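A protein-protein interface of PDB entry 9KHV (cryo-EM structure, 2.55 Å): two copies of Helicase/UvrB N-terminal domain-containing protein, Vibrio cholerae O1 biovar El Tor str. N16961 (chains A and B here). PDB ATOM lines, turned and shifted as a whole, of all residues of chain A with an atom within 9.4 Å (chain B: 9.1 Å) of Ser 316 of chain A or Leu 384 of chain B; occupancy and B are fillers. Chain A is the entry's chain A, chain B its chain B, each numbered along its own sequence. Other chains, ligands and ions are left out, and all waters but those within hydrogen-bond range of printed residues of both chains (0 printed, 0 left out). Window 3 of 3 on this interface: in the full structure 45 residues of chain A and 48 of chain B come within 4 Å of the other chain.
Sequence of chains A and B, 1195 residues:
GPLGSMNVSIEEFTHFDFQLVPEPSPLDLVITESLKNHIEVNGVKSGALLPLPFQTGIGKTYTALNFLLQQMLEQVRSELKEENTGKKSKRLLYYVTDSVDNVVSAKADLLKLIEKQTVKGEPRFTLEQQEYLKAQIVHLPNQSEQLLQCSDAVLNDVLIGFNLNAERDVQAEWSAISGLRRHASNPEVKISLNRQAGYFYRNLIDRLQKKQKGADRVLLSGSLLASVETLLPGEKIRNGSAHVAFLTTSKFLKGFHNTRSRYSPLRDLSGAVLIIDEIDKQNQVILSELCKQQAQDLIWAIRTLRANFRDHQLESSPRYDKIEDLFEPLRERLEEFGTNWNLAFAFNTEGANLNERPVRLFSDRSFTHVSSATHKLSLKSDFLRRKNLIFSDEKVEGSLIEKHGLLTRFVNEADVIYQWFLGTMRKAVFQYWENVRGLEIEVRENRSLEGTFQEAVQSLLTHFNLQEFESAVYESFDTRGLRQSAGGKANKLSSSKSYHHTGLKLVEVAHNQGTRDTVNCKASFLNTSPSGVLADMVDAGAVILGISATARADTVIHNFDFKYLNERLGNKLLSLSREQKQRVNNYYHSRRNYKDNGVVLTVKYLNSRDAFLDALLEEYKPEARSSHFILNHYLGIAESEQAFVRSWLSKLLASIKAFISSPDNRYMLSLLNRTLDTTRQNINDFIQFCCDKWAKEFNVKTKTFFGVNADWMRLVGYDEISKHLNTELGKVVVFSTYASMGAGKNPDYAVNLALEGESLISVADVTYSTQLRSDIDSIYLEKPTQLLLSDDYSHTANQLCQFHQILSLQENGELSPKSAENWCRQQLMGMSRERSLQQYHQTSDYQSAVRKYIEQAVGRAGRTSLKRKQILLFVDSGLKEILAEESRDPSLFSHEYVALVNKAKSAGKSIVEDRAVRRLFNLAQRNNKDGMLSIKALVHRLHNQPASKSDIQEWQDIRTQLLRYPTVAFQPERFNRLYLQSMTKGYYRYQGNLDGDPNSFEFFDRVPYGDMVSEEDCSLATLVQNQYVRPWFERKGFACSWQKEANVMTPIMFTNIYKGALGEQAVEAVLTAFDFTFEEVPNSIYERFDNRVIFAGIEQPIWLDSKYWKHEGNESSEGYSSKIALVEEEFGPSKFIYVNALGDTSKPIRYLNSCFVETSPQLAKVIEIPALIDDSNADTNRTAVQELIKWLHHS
The side-chain carboxylate of Glu 315 of chain A is in salt-bridge range of the guanidinium group of Arg 385 of chain B (3.8 Å).
The side-chain hydroxyl of Ser 316 of chain A lies within hydrogen-bond range of the backbone carbonyl oxygen of Leu 384 of chain B (2.8 Å).
The side-chain hydroxyl (OG) of Ser 316 of chain A is in hydrogen-bond range of the backbone carbonyl oxygen (O) of Arg 385 of chain B (3.0 Å).
The side-chain carboxylate of Asp 517 of chain B sits close to the side-chain hydroxyl of Tyr 320 of chain A, at 3.3 Å.
A ring nitrogen (NE2) of His 463 of chain A lies within hydrogen-bond range of the side-chain amino group (NZ) of Lys 387 of chain B (2.8 Å).
OE1 of Glu 315 of chain A lies close to OG of Ser 317 of chain A.
The backbone carbonyl oxygen (O) of Lys 387 of chain B sits at hydrogen-bond distance from the backbone NH (N) of Asp 382 of chain B, at 2.9 Å.
O of Asp 517 of chain B lies within hydrogen-bond range of NZ of Lys 387 of chain B.
Gln 313 of chain A touches Arg 386 of chain B (OE1 to NH1, 3.5 Å).
Arg 386 of chain B touches Leu 314 of chain A (CB to O, 3.7 Å).
Glu 315 of chain A touches Arg 386 of chain B.
CD of Lys 387 of chain B touches CG of Glu 315 of chain A, 3.8 Å away.
Glu 315 of chain A touches Asp 517 of chain B (OE1 to OD2, 3.9 Å).
Asp 517 of chain B touches His 463 of chain A (OD2 to CE1, 3.3 Å).
Of the printed residues of chain B, Leu 314 of chain A touches Arg 386.
Ser 317 of chain A touches none of the printed residues of chain B.
Of the printed residues of chain B, Tyr 320 of chain A touches Asp 517.
Lys 380 of chain B touches none of the printed residues of chain A.
Leu 384 of chain B touches just one residue of chain A: Ser 316 (2.8 Å).
Printed residues of chain A within 4 Å of Arg 386 of chain B: Gln 313, Leu 314 and Glu 315.
The nearest residue of chain B that does not touch Ser 316 of chain A is Arg 386 of chain B (4.1 Å).
The nearest residue of chain A that does not touch Leu 384 of chain B is Glu 315 of chain A (6.7 Å).
Of the 13 printed residues of chain A, 6 touch a printed residue of chain B.
Printed residues of chain B that touch a printed residue of chain A: Leu 384, Arg 385, Arg 386, Lys 387 and Asp 517.
Along chain B the printed residues that touch a printed residue of chain A span positions 384 to 517.
Among the printed residues, 11 pairs touch across the chains.
No position is printed for both chains.
Of the 11 pairs that touch across the chains among the printed residues, none has its exchanged pair printed and touching as well.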
ATOM      1  N   GLN A 313      26.155  -9.832  -9.668  1.00  0.00           N
ATOM      2  CA  GLN A 313      26.311  -9.171  -8.381  1.00  0.00           C
ATOM      3  C   GLN A 313      25.124  -8.264  -8.096  1.00  0.00           C
ATOM      4  O   GLN A 313      24.454  -7.782  -9.012  1.00  0.00           O
ATOM      5  CB  GLN A 313      27.591  -8.330  -8.330  1.00  0.00           C
ATOM      6  CG  GLN A 313      28.799  -8.998  -8.932  1.00  0.00           C
ATOM      7  CD  GLN A 313      29.846  -9.331  -7.901  1.00  0.00           C
ATOM      8  OE1 GLN A 313      30.335  -8.453  -7.194  1.00  0.00           O
ATOM      9  NE2 GLN A 313      30.191 -10.608  -7.799  1.00  0.00           N
ATOM     10  N   LEU A 314      24.879  -8.036  -6.809  1.00  0.00           N
ATOM     11  CA  LEU A 314      23.920  -7.041  -6.368  1.00  0.00           C
ATOM     12  C   LEU A 314      24.553  -5.655  -6.365  1.00  0.00           C
ATOM     13  O   LEU A 314      25.772  -5.498  -6.265  1.00  0.00           O
ATOM     14  CB  LEU A 314      23.405  -7.363  -4.966  1.00  0.00           C
ATOM     15  CG  LEU A 314      22.196  -8.279  -4.808  1.00  0.00           C
ATOM     16  CD1 LEU A 314      22.096  -8.738  -3.370  1.00  0.00           C
ATOM     17  CD2 LEU A 314      20.933  -7.560  -5.216  1.00  0.00           C
ATOM     18  N   GLU A 315      23.703  -4.642  -6.473  1.00  0.00           N
ATOM     19  CA  GLU A 315      24.144  -3.265  -6.328  1.00  0.00           C
ATOM     20  C   GLU A 315      24.488  -2.980  -4.871  1.00  0.00           C
ATOM     21  O   GLU A 315      23.914  -3.568  -3.951  1.00  0.00           O
ATOM     22  CB  GLU A 315      23.059  -2.309  -6.814  1.00  0.00           C
ATOM     23  CG  GLU A 315      23.541  -0.904  -7.088  1.00  0.00           C
ATOM     24  CD  GLU A 315      22.548   0.144  -6.644  1.00  0.00           C
ATOM     25  OE1 GLU A 315      21.360  -0.196  -6.481  1.00  0.00           O
ATOM     26  OE2 GLU A 315      22.955   1.310  -6.464  1.00  0.00           O
ATOM     27  N   SER A 316      25.433  -2.062  -4.663  1.00  0.00           N
ATOM     28  CA  SER A 316      25.885  -1.711  -3.322  1.00  0.00           C
ATOM     29  C   SER A 316      25.165  -0.493  -2.759  1.00  0.00           C
ATOM     30  O   SER A 316      25.764   0.286  -2.007  1.00  0.00           O
ATOM     31  CB  SER A 316      27.397  -1.487  -3.316  1.00  0.00           C
ATOM     32  OG  SER A 316      27.784  -0.593  -4.339  1.00  0.00           O
ATOM     33  N   SER A 317      23.895  -0.305  -3.106  1.00  0.00           N
ATOM     34  CA  SER A 317      23.101   0.766  -2.535  1.00  0.00           C
ATOM     35  C   SER A 317      22.701   0.420  -1.102  1.00  0.00           C
ATOM     36  O   SER A 317      22.783  -0.738  -0.687  1.00  0.00           O
ATOM     37  CB  SER A 317      21.857   1.010  -3.386  1.00  0.00           C
ATOM     38  OG  SER A 317      20.843   0.073  -3.082  1.00  0.00           O
ATOM     39  N   PRO A 318      22.285   1.417  -0.315  1.00  0.00           N
ATOM     40  CA  PRO A 318      21.842   1.127   1.058  1.00  0.00           C
ATOM     41  C   PRO A 318      20.631   0.213   1.144  1.00  0.00           C
ATOM     42  O   PRO A 318      20.418  -0.396   2.199  1.00  0.00           O
ATOM     43  CB  PRO A 318      21.529   2.519   1.621  1.00  0.00           C
ATOM     44  CG  PRO A 318      22.415   3.425   0.853  1.00  0.00           C
ATOM     45  CD  PRO A 318      22.447   2.864  -0.539  1.00  0.00           C
ATOM     46  N   ARG A 319      19.824   0.100   0.088  1.00  0.00           N
ATOM     47  CA  ARG A 319      18.685  -0.812   0.137  1.00  0.00           C
ATOM     48  C   ARG A 319      19.129  -2.266   0.209  1.00  0.00           C
ATOM     49  O   ARG A 319      18.388  -3.112   0.721  1.00  0.00           O
ATOM     50  CB  ARG A 319      17.779  -0.613  -1.076  1.00  0.00           C
ATOM     51  CG  ARG A 319      17.903   0.729  -1.761  1.00  0.00           C
ATOM     52  CD  ARG A 319      17.340   0.656  -3.172  1.00  0.00           C
ATOM     53  NE  ARG A 319      15.933   0.275  -3.180  1.00  0.00           N
ATOM     54  CZ  ARG A 319      14.931   1.092  -2.886  1.00  0.00           C
ATOM     55  NH1 ARG A 319      15.143   2.360  -2.570  1.00  0.00           N
ATOM     56  NH2 ARG A 319      13.686   0.628  -2.912  1.00  0.00           N
ATOM     57  N   TYR A 320      20.321  -2.579  -0.301  1.00  0.00           N
ATOM     58  CA  TYR A 320      20.845  -3.937  -0.313  1.00  0.00           C
ATOM     59  C   TYR A 320      21.940  -4.143   0.725  1.00  0.00           C
ATOM     60  O   TYR A 320      22.835  -4.971   0.526  1.00  0.00           O
ATOM     61  CB  TYR A 320      21.362  -4.293  -1.705  1.00  0.00           C
ATOM     62  CG  TYR A 320      20.343  -4.085  -2.796  1.00  0.00           C
ATOM     63  CD1 TYR A 320      19.323  -5.001  -2.999  1.00  0.00           C
ATOM     64  CD2 TYR A 320      20.397  -2.971  -3.619  1.00  0.00           C
ATOM     65  CE1 TYR A 320      18.387  -4.813  -3.991  1.00  0.00           C
ATOM     66  CE2 TYR A 320      19.464  -2.775  -4.612  1.00  0.00           C
ATOM     67  CZ  TYR A 320      18.462  -3.701  -4.793  1.00  0.00           C
ATOM     68  OH  TYR A 320      17.529  -3.513  -5.783  1.00  0.00           O
ATOM     69  N   ASP A 321      21.887  -3.403   1.828  1.00  0.00           N
ATOM     70  CA  ASP A 321      22.893  -3.531   2.871  1.00  0.00           C
ATOM     71  C   ASP A 321      22.855  -4.928   3.477  1.00  0.00           C
ATOM     72  O   ASP A 321      21.782  -5.453   3.783  1.00  0.00           O
ATOM     73  CB  ASP A 321      22.670  -2.475   3.950  1.00  0.00           C
ATOM     74  CG  ASP A 321      23.699  -2.548   5.058  1.00  0.00           C
ATOM     75  OD1 ASP A 321      24.899  -2.355   4.770  1.00  0.00           O
ATOM     76  OD2 ASP A 321      23.309  -2.794   6.218  1.00  0.00           O
ATOM     77  N   LYS A 322      24.033  -5.532   3.623  1.00  0.00           N
ATOM     78  CA  LYS A 322      24.261  -6.842   4.232  1.00  0.00           C
ATOM     79  C   LYS A 322      23.411  -7.955   3.621  1.00  0.00           C
ATOM     80  O   LYS A 322      23.271  -9.025   4.224  1.00  0.00           O
ATOM     81  CB  LYS A 322      24.080  -6.779   5.758  1.00  0.00           C
ATOM     82  CG  LYS A 322      22.667  -6.923   6.288  1.00  0.00           C
ATOM     83  CD  LYS A 322      22.654  -6.855   7.803  1.00  0.00           C
ATOM     84  CE  LYS A 322      23.371  -5.612   8.294  1.00  0.00           C
ATOM     85  NZ  LYS A 322      22.635  -4.372   7.923  1.00  0.00           N
ATOM     86  N   ILE A 323      22.878  -7.751   2.416  1.00  0.00           N
ATOM     87  CA  ILE A 323      22.154  -8.818   1.732  1.00  0.00           C
ATOM     88  C   ILE A 323      23.117  -9.686   0.932  1.00  0.00           C
ATOM     89  O   ILE A 323      22.931 -10.903   0.819  1.00  0.00           O
ATOM     90  CB  ILE A 323      21.049  -8.223   0.840  1.00  0.00           C
ATOM     91  CG1 ILE A 323      19.960  -7.579   1.694  1.00  0.00           C
ATOM     92  CG2 ILE A 323      20.441  -9.286  -0.052  1.00  0.00           C
ATOM     93  CD1 ILE A 323      18.824  -7.009   0.890  1.00  0.00           C
ATOM     94  N   GLU A 324      24.165  -9.079   0.372  1.00  0.00           N
ATOM     95  CA  GLU A 324      25.128  -9.838  -0.418  1.00  0.00           C
ATOM     96  C   GLU A 324      25.856 -10.876   0.424  1.00  0.00           C
ATOM     97  O   GLU A 324      26.236 -11.934  -0.091  1.00  0.00           O
ATOM     98  CB  GLU A 324      26.128  -8.885  -1.076  1.00  0.00           C
ATOM     99  CG  GLU A 324      27.086  -9.549  -2.052  1.00  0.00           C
ATOM    100  CD  GLU A 324      26.507  -9.696  -3.449  1.00  0.00           C
ATOM    101  OE1 GLU A 324      25.409 -10.276  -3.586  1.00  0.00           O
ATOM    102  OE2 GLU A 324      27.152  -9.236  -4.415  1.00  0.00           O
ATOM    103  N   HIS A 463      18.506  -8.668 -10.290  1.00  0.00           N
ATOM    104  CA  HIS A 463      19.933  -8.411 -10.131  1.00  0.00           C
ATOM    105  C   HIS A 463      20.752  -9.665 -10.407  1.00  0.00           C
ATOM    106  O   HIS A 463      21.854  -9.586 -10.959  1.00  0.00           O
ATOM    107  CB  HIS A 463      20.226  -7.882  -8.732  1.00  0.00           C
ATOM    108  CG  HIS A 463      20.112  -6.397  -8.615  1.00  0.00           C
ATOM    109  ND1 HIS A 463      18.916  -5.762  -8.364  1.00  0.00           N
ATOM    110  CD2 HIS A 463      21.043  -5.421  -8.718  1.00  0.00           C
ATOM    111  CE1 HIS A 463      19.115  -4.459  -8.317  1.00  0.00           C
ATOM    112  NE2 HIS A 463      20.398  -4.226  -8.523  1.00  0.00           N
ATOM    113  N   PHE B 345      27.060  -6.670 -13.792  1.00  0.00           N
ATOM    114  CA  PHE B 345      26.171  -5.723 -13.141  1.00  0.00           C
ATOM    115  C   PHE B 345      24.849  -5.628 -13.891  1.00  0.00           C
ATOM    116  O   PHE B 345      24.765  -5.899 -15.091  1.00  0.00           O
ATOM    117  CB  PHE B 345      26.810  -4.334 -13.061  1.00  0.00           C
ATOM    118  CG  PHE B 345      28.210  -4.334 -12.528  1.00  0.00           C
ATOM    119  CD1 PHE B 345      28.575  -5.168 -11.487  1.00  0.00           C
ATOM    120  CD2 PHE B 345      29.161  -3.490 -13.066  1.00  0.00           C
ATOM    121  CE1 PHE B 345      29.861  -5.163 -11.000  1.00  0.00           C
ATOM    122  CE2 PHE B 345      30.447  -3.479 -12.581  1.00  0.00           C
ATOM    123  CZ  PHE B 345      30.798  -4.318 -11.548  1.00  0.00           C
ATOM    124  N   LYS B 380      27.725   3.886 -18.715  1.00  0.00           N
ATOM    125  CA  LYS B 380      28.946   3.837 -17.924  1.00  0.00           C
ATOM    126  C   LYS B 380      28.816   2.789 -16.830  1.00  0.00           C
ATOM    127  O   LYS B 380      27.774   2.681 -16.184  1.00  0.00           O
ATOM    128  CB  LYS B 380      29.256   5.208 -17.308  1.00  0.00           C
ATOM    129  CG  LYS B 380      29.759   5.154 -15.881  1.00  0.00           C
ATOM    130  CD  LYS B 380      30.156   6.525 -15.378  1.00  0.00           C
ATOM    131  CE  LYS B 380      28.942   7.325 -14.956  1.00  0.00           C
ATOM    132  NZ  LYS B 380      29.324   8.654 -14.407  1.00  0.00           N
ATOM    133  N   SER B 381      29.881   2.024 -16.620  1.00  0.00           N
ATOM    134  CA  SER B 381      29.917   1.038 -15.548  1.00  0.00           C
ATOM    135  C   SER B 381      30.493   1.680 -14.294  1.00  0.00           C
ATOM    136  O   SER B 381      31.649   2.113 -14.287  1.00  0.00           O
ATOM    137  CB  SER B 381      30.741  -0.180 -15.953  1.00  0.00           C
ATOM    138  OG  SER B 381      29.966  -1.075 -16.730  1.00  0.00           O
ATOM    139  N   ASP B 382      29.685   1.742 -13.240  1.00  0.00           N
ATOM    140  CA  ASP B 382      30.117   2.232 -11.940  1.00  0.00           C
ATOM    141  C   ASP B 382      30.536   1.026 -11.109  1.00  0.00           C
ATOM    142  O   ASP B 382      29.690   0.233 -10.680  1.00  0.00           O
ATOM    143  CB  ASP B 382      29.004   3.019 -11.255  1.00  0.00           C
ATOM    144  CG  ASP B 382      29.536   4.059 -10.297  1.00  0.00           C
ATOM    145  OD1 ASP B 382      30.735   3.997  -9.957  1.00  0.00           O
ATOM    146  OD2 ASP B 382      28.756   4.940  -9.883  1.00  0.00           O
ATOM    147  N   PHE B 383      31.847   0.881 -10.906  1.00  0.00           N
ATOM    148  CA  PHE B 383      32.364  -0.252 -10.149  1.00  0.00           C
ATOM    149  C   PHE B 383      32.154  -0.071  -8.654  1.00  0.00           C
ATOM    150  O   PHE B 383      31.994  -1.060  -7.930  1.00  0.00           O
ATOM    151  CB  PHE B 383      33.846  -0.452 -10.458  1.00  0.00           C
ATOM    152  CG  PHE B 383      34.105  -1.084 -11.792  1.00  0.00           C
ATOM    153  CD1 PHE B 383      33.932  -0.361 -12.958  1.00  0.00           C
ATOM    154  CD2 PHE B 383      34.516  -2.401 -11.881  1.00  0.00           C
ATOM    155  CE1 PHE B 383      34.165  -0.938 -14.187  1.00  0.00           C
ATOM    156  CE2 PHE B 383      34.753  -2.983 -13.108  1.00  0.00           C
ATOM    157  CZ  PHE B 383      34.577  -2.249 -14.262  1.00  0.00           C
ATOM    158  N   LEU B 384      32.165   1.172  -8.174  1.00  0.00           N
ATOM    159  CA  LEU B 384      31.900   1.418  -6.761  1.00  0.00           C
ATOM    160  C   LEU B 384      30.457   1.086  -6.407  1.00  0.00           C
ATOM    161  O   LEU B 384      30.193   0.469  -5.369  1.00  0.00           O
ATOM    162  CB  LEU B 384      32.221   2.871  -6.413  1.00  0.00           C
ATOM    163  CG  LEU B 384      32.035   3.269  -4.948  1.00  0.00           C
ATOM    164  CD1 LEU B 384      33.380   3.415  -4.259  1.00  0.00           C
ATOM    165  CD2 LEU B 384      31.231   4.555  -4.842  1.00  0.00           C
ATOM    166  N   ARG B 385      29.513   1.484  -7.256  1.00  0.00           N
ATOM    167  CA  ARG B 385      28.114   1.137  -7.059  1.00  0.00           C
ATOM    168  C   ARG B 385      27.776  -0.263  -7.545  1.00  0.00           C
ATOM    169  O   ARG B 385      26.715  -0.779  -7.184  1.00  0.00           O
ATOM    170  CB  ARG B 385      27.210   2.138  -7.776  1.00  0.00           C
ATOM    171  CG  ARG B 385      26.904   3.393  -6.992  1.00  0.00           C
ATOM    172  CD  ARG B 385      26.238   4.419  -7.886  1.00  0.00           C
ATOM    173  NE  ARG B 385      24.853   4.062  -8.165  1.00  0.00           N
ATOM    174  CZ  ARG B 385      23.920   4.922  -8.549  1.00  0.00           C
ATOM    175  NH1 ARG B 385      24.188   6.206  -8.715  1.00  0.00           N
ATOM    176  NH2 ARG B 385      22.686   4.481  -8.776  1.00  0.00           N
ATOM    177  N   ARG B 386      28.647  -0.881  -8.344  1.00  0.00           N
ATOM    178  CA  ARG B 386      28.364  -2.165  -8.986  1.00  0.00           C
ATOM    179  C   ARG B 386      27.087  -2.079  -9.819  1.00  0.00           C
ATOM    180  O   ARG B 386      26.116  -2.800  -9.592  1.00  0.00           O
ATOM    181  CB  ARG B 386      28.281  -3.293  -7.958  1.00  0.00           C
ATOM    182  CG  ARG B 386      29.562  -3.515  -7.182  1.00  0.00           C
ATOM    183  CD  ARG B 386      29.618  -4.921  -6.628  1.00  0.00           C
ATOM    184  NE  ARG B 386      29.574  -4.937  -5.172  1.00  0.00           N
ATOM    185  CZ  ARG B 386      30.500  -5.487  -4.402  1.00  0.00           C
ATOM    186  NH1 ARG B 386      31.564  -6.080  -4.917  1.00  0.00           N
ATOM    187  NH2 ARG B 386      30.356  -5.443  -3.081  1.00  0.00           N
ATOM    188  N   LYS B 387      27.101  -1.182 -10.801  1.00  0.00           N
ATOM    189  CA  LYS B 387      25.919  -0.874 -11.592  1.00  0.00           C
ATOM    190  C   LYS B 387      26.341  -0.482 -12.999  1.00  0.00           C
ATOM    191  O   LYS B 387      27.490  -0.109 -13.232  1.00  0.00           O
ATOM    192  CB  LYS B 387      25.115   0.262 -10.949  1.00  0.00           C
ATOM    193  CG  LYS B 387      23.618   0.206 -11.171  1.00  0.00           C
ATOM    194  CD  LYS B 387      23.039  -1.158 -10.873  1.00  0.00           C
ATOM    195  CE  LYS B 387      21.552  -1.153 -11.152  1.00  0.00           C
ATOM    196  NZ  LYS B 387      20.860  -2.328 -10.591  1.00  0.00           N
ATOM    197  N   ASN B 388      25.405  -0.576 -13.940  1.00  0.00           N
ATOM    198  CA  ASN B 388      25.590  -0.054 -15.290  1.00  0.00           C
ATOM    199  C   ASN B 388      24.563   1.050 -15.488  1.00  0.00           C
ATOM    200  O   ASN B 388      23.370   0.774 -15.640  1.00  0.00           O
ATOM    201  CB  ASN B 388      25.434  -1.154 -16.335  1.00  0.00           C
ATOM    202  CG  ASN B 388      26.616  -2.091 -16.377  1.00  0.00           C
ATOM    203  OD1 ASN B 388      27.760  -1.668 -16.240  1.00  0.00           O
ATOM    204  ND2 ASN B 388      26.347  -3.372 -16.571  1.00  0.00           N
ATOM    205  N   LEU B 389      25.022   2.293 -15.494  1.00  0.00           N
ATOM    206  CA  LEU B 389      24.148   3.452 -15.455  1.00  0.00           C
ATOM    207  C   LEU B 389      24.049   4.096 -16.829  1.00  0.00           C
ATOM    208  O   LEU B 389      25.048   4.226 -17.545  1.00  0.00           O
ATOM    209  CB  LEU B 389      24.656   4.464 -14.429  1.00  0.00           C
ATOM    210  CG  LEU B 389      24.795   3.856 -13.034  1.00  0.00           C
ATOM    211  CD1 LEU B 389      25.736   4.668 -12.172  1.00  0.00           C
ATOM    212  CD2 LEU B 389      23.435   3.734 -12.379  1.00  0.00           C
ATOM    213  N   ASP B 517      14.725   0.146  -9.563  1.00  0.00           N
ATOM    214  CA  ASP B 517      16.156   0.396  -9.656  1.00  0.00           C
ATOM    215  C   ASP B 517      16.836  -0.427 -10.743  1.00  0.00           C
ATOM    216  O   ASP B 517      18.069  -0.451 -10.801  1.00  0.00           O
ATOM    217  CB  ASP B 517      16.835   0.145  -8.303  1.00  0.00           C
ATOM    218  CG  ASP B 517      16.863  -1.317  -7.925  1.00  0.00           C
ATOM    219  OD1 ASP B 517      15.970  -2.070  -8.365  1.00  0.00           O
ATOM    220  OD2 ASP B 517      17.781  -1.714  -7.180  1.00  0.00           O
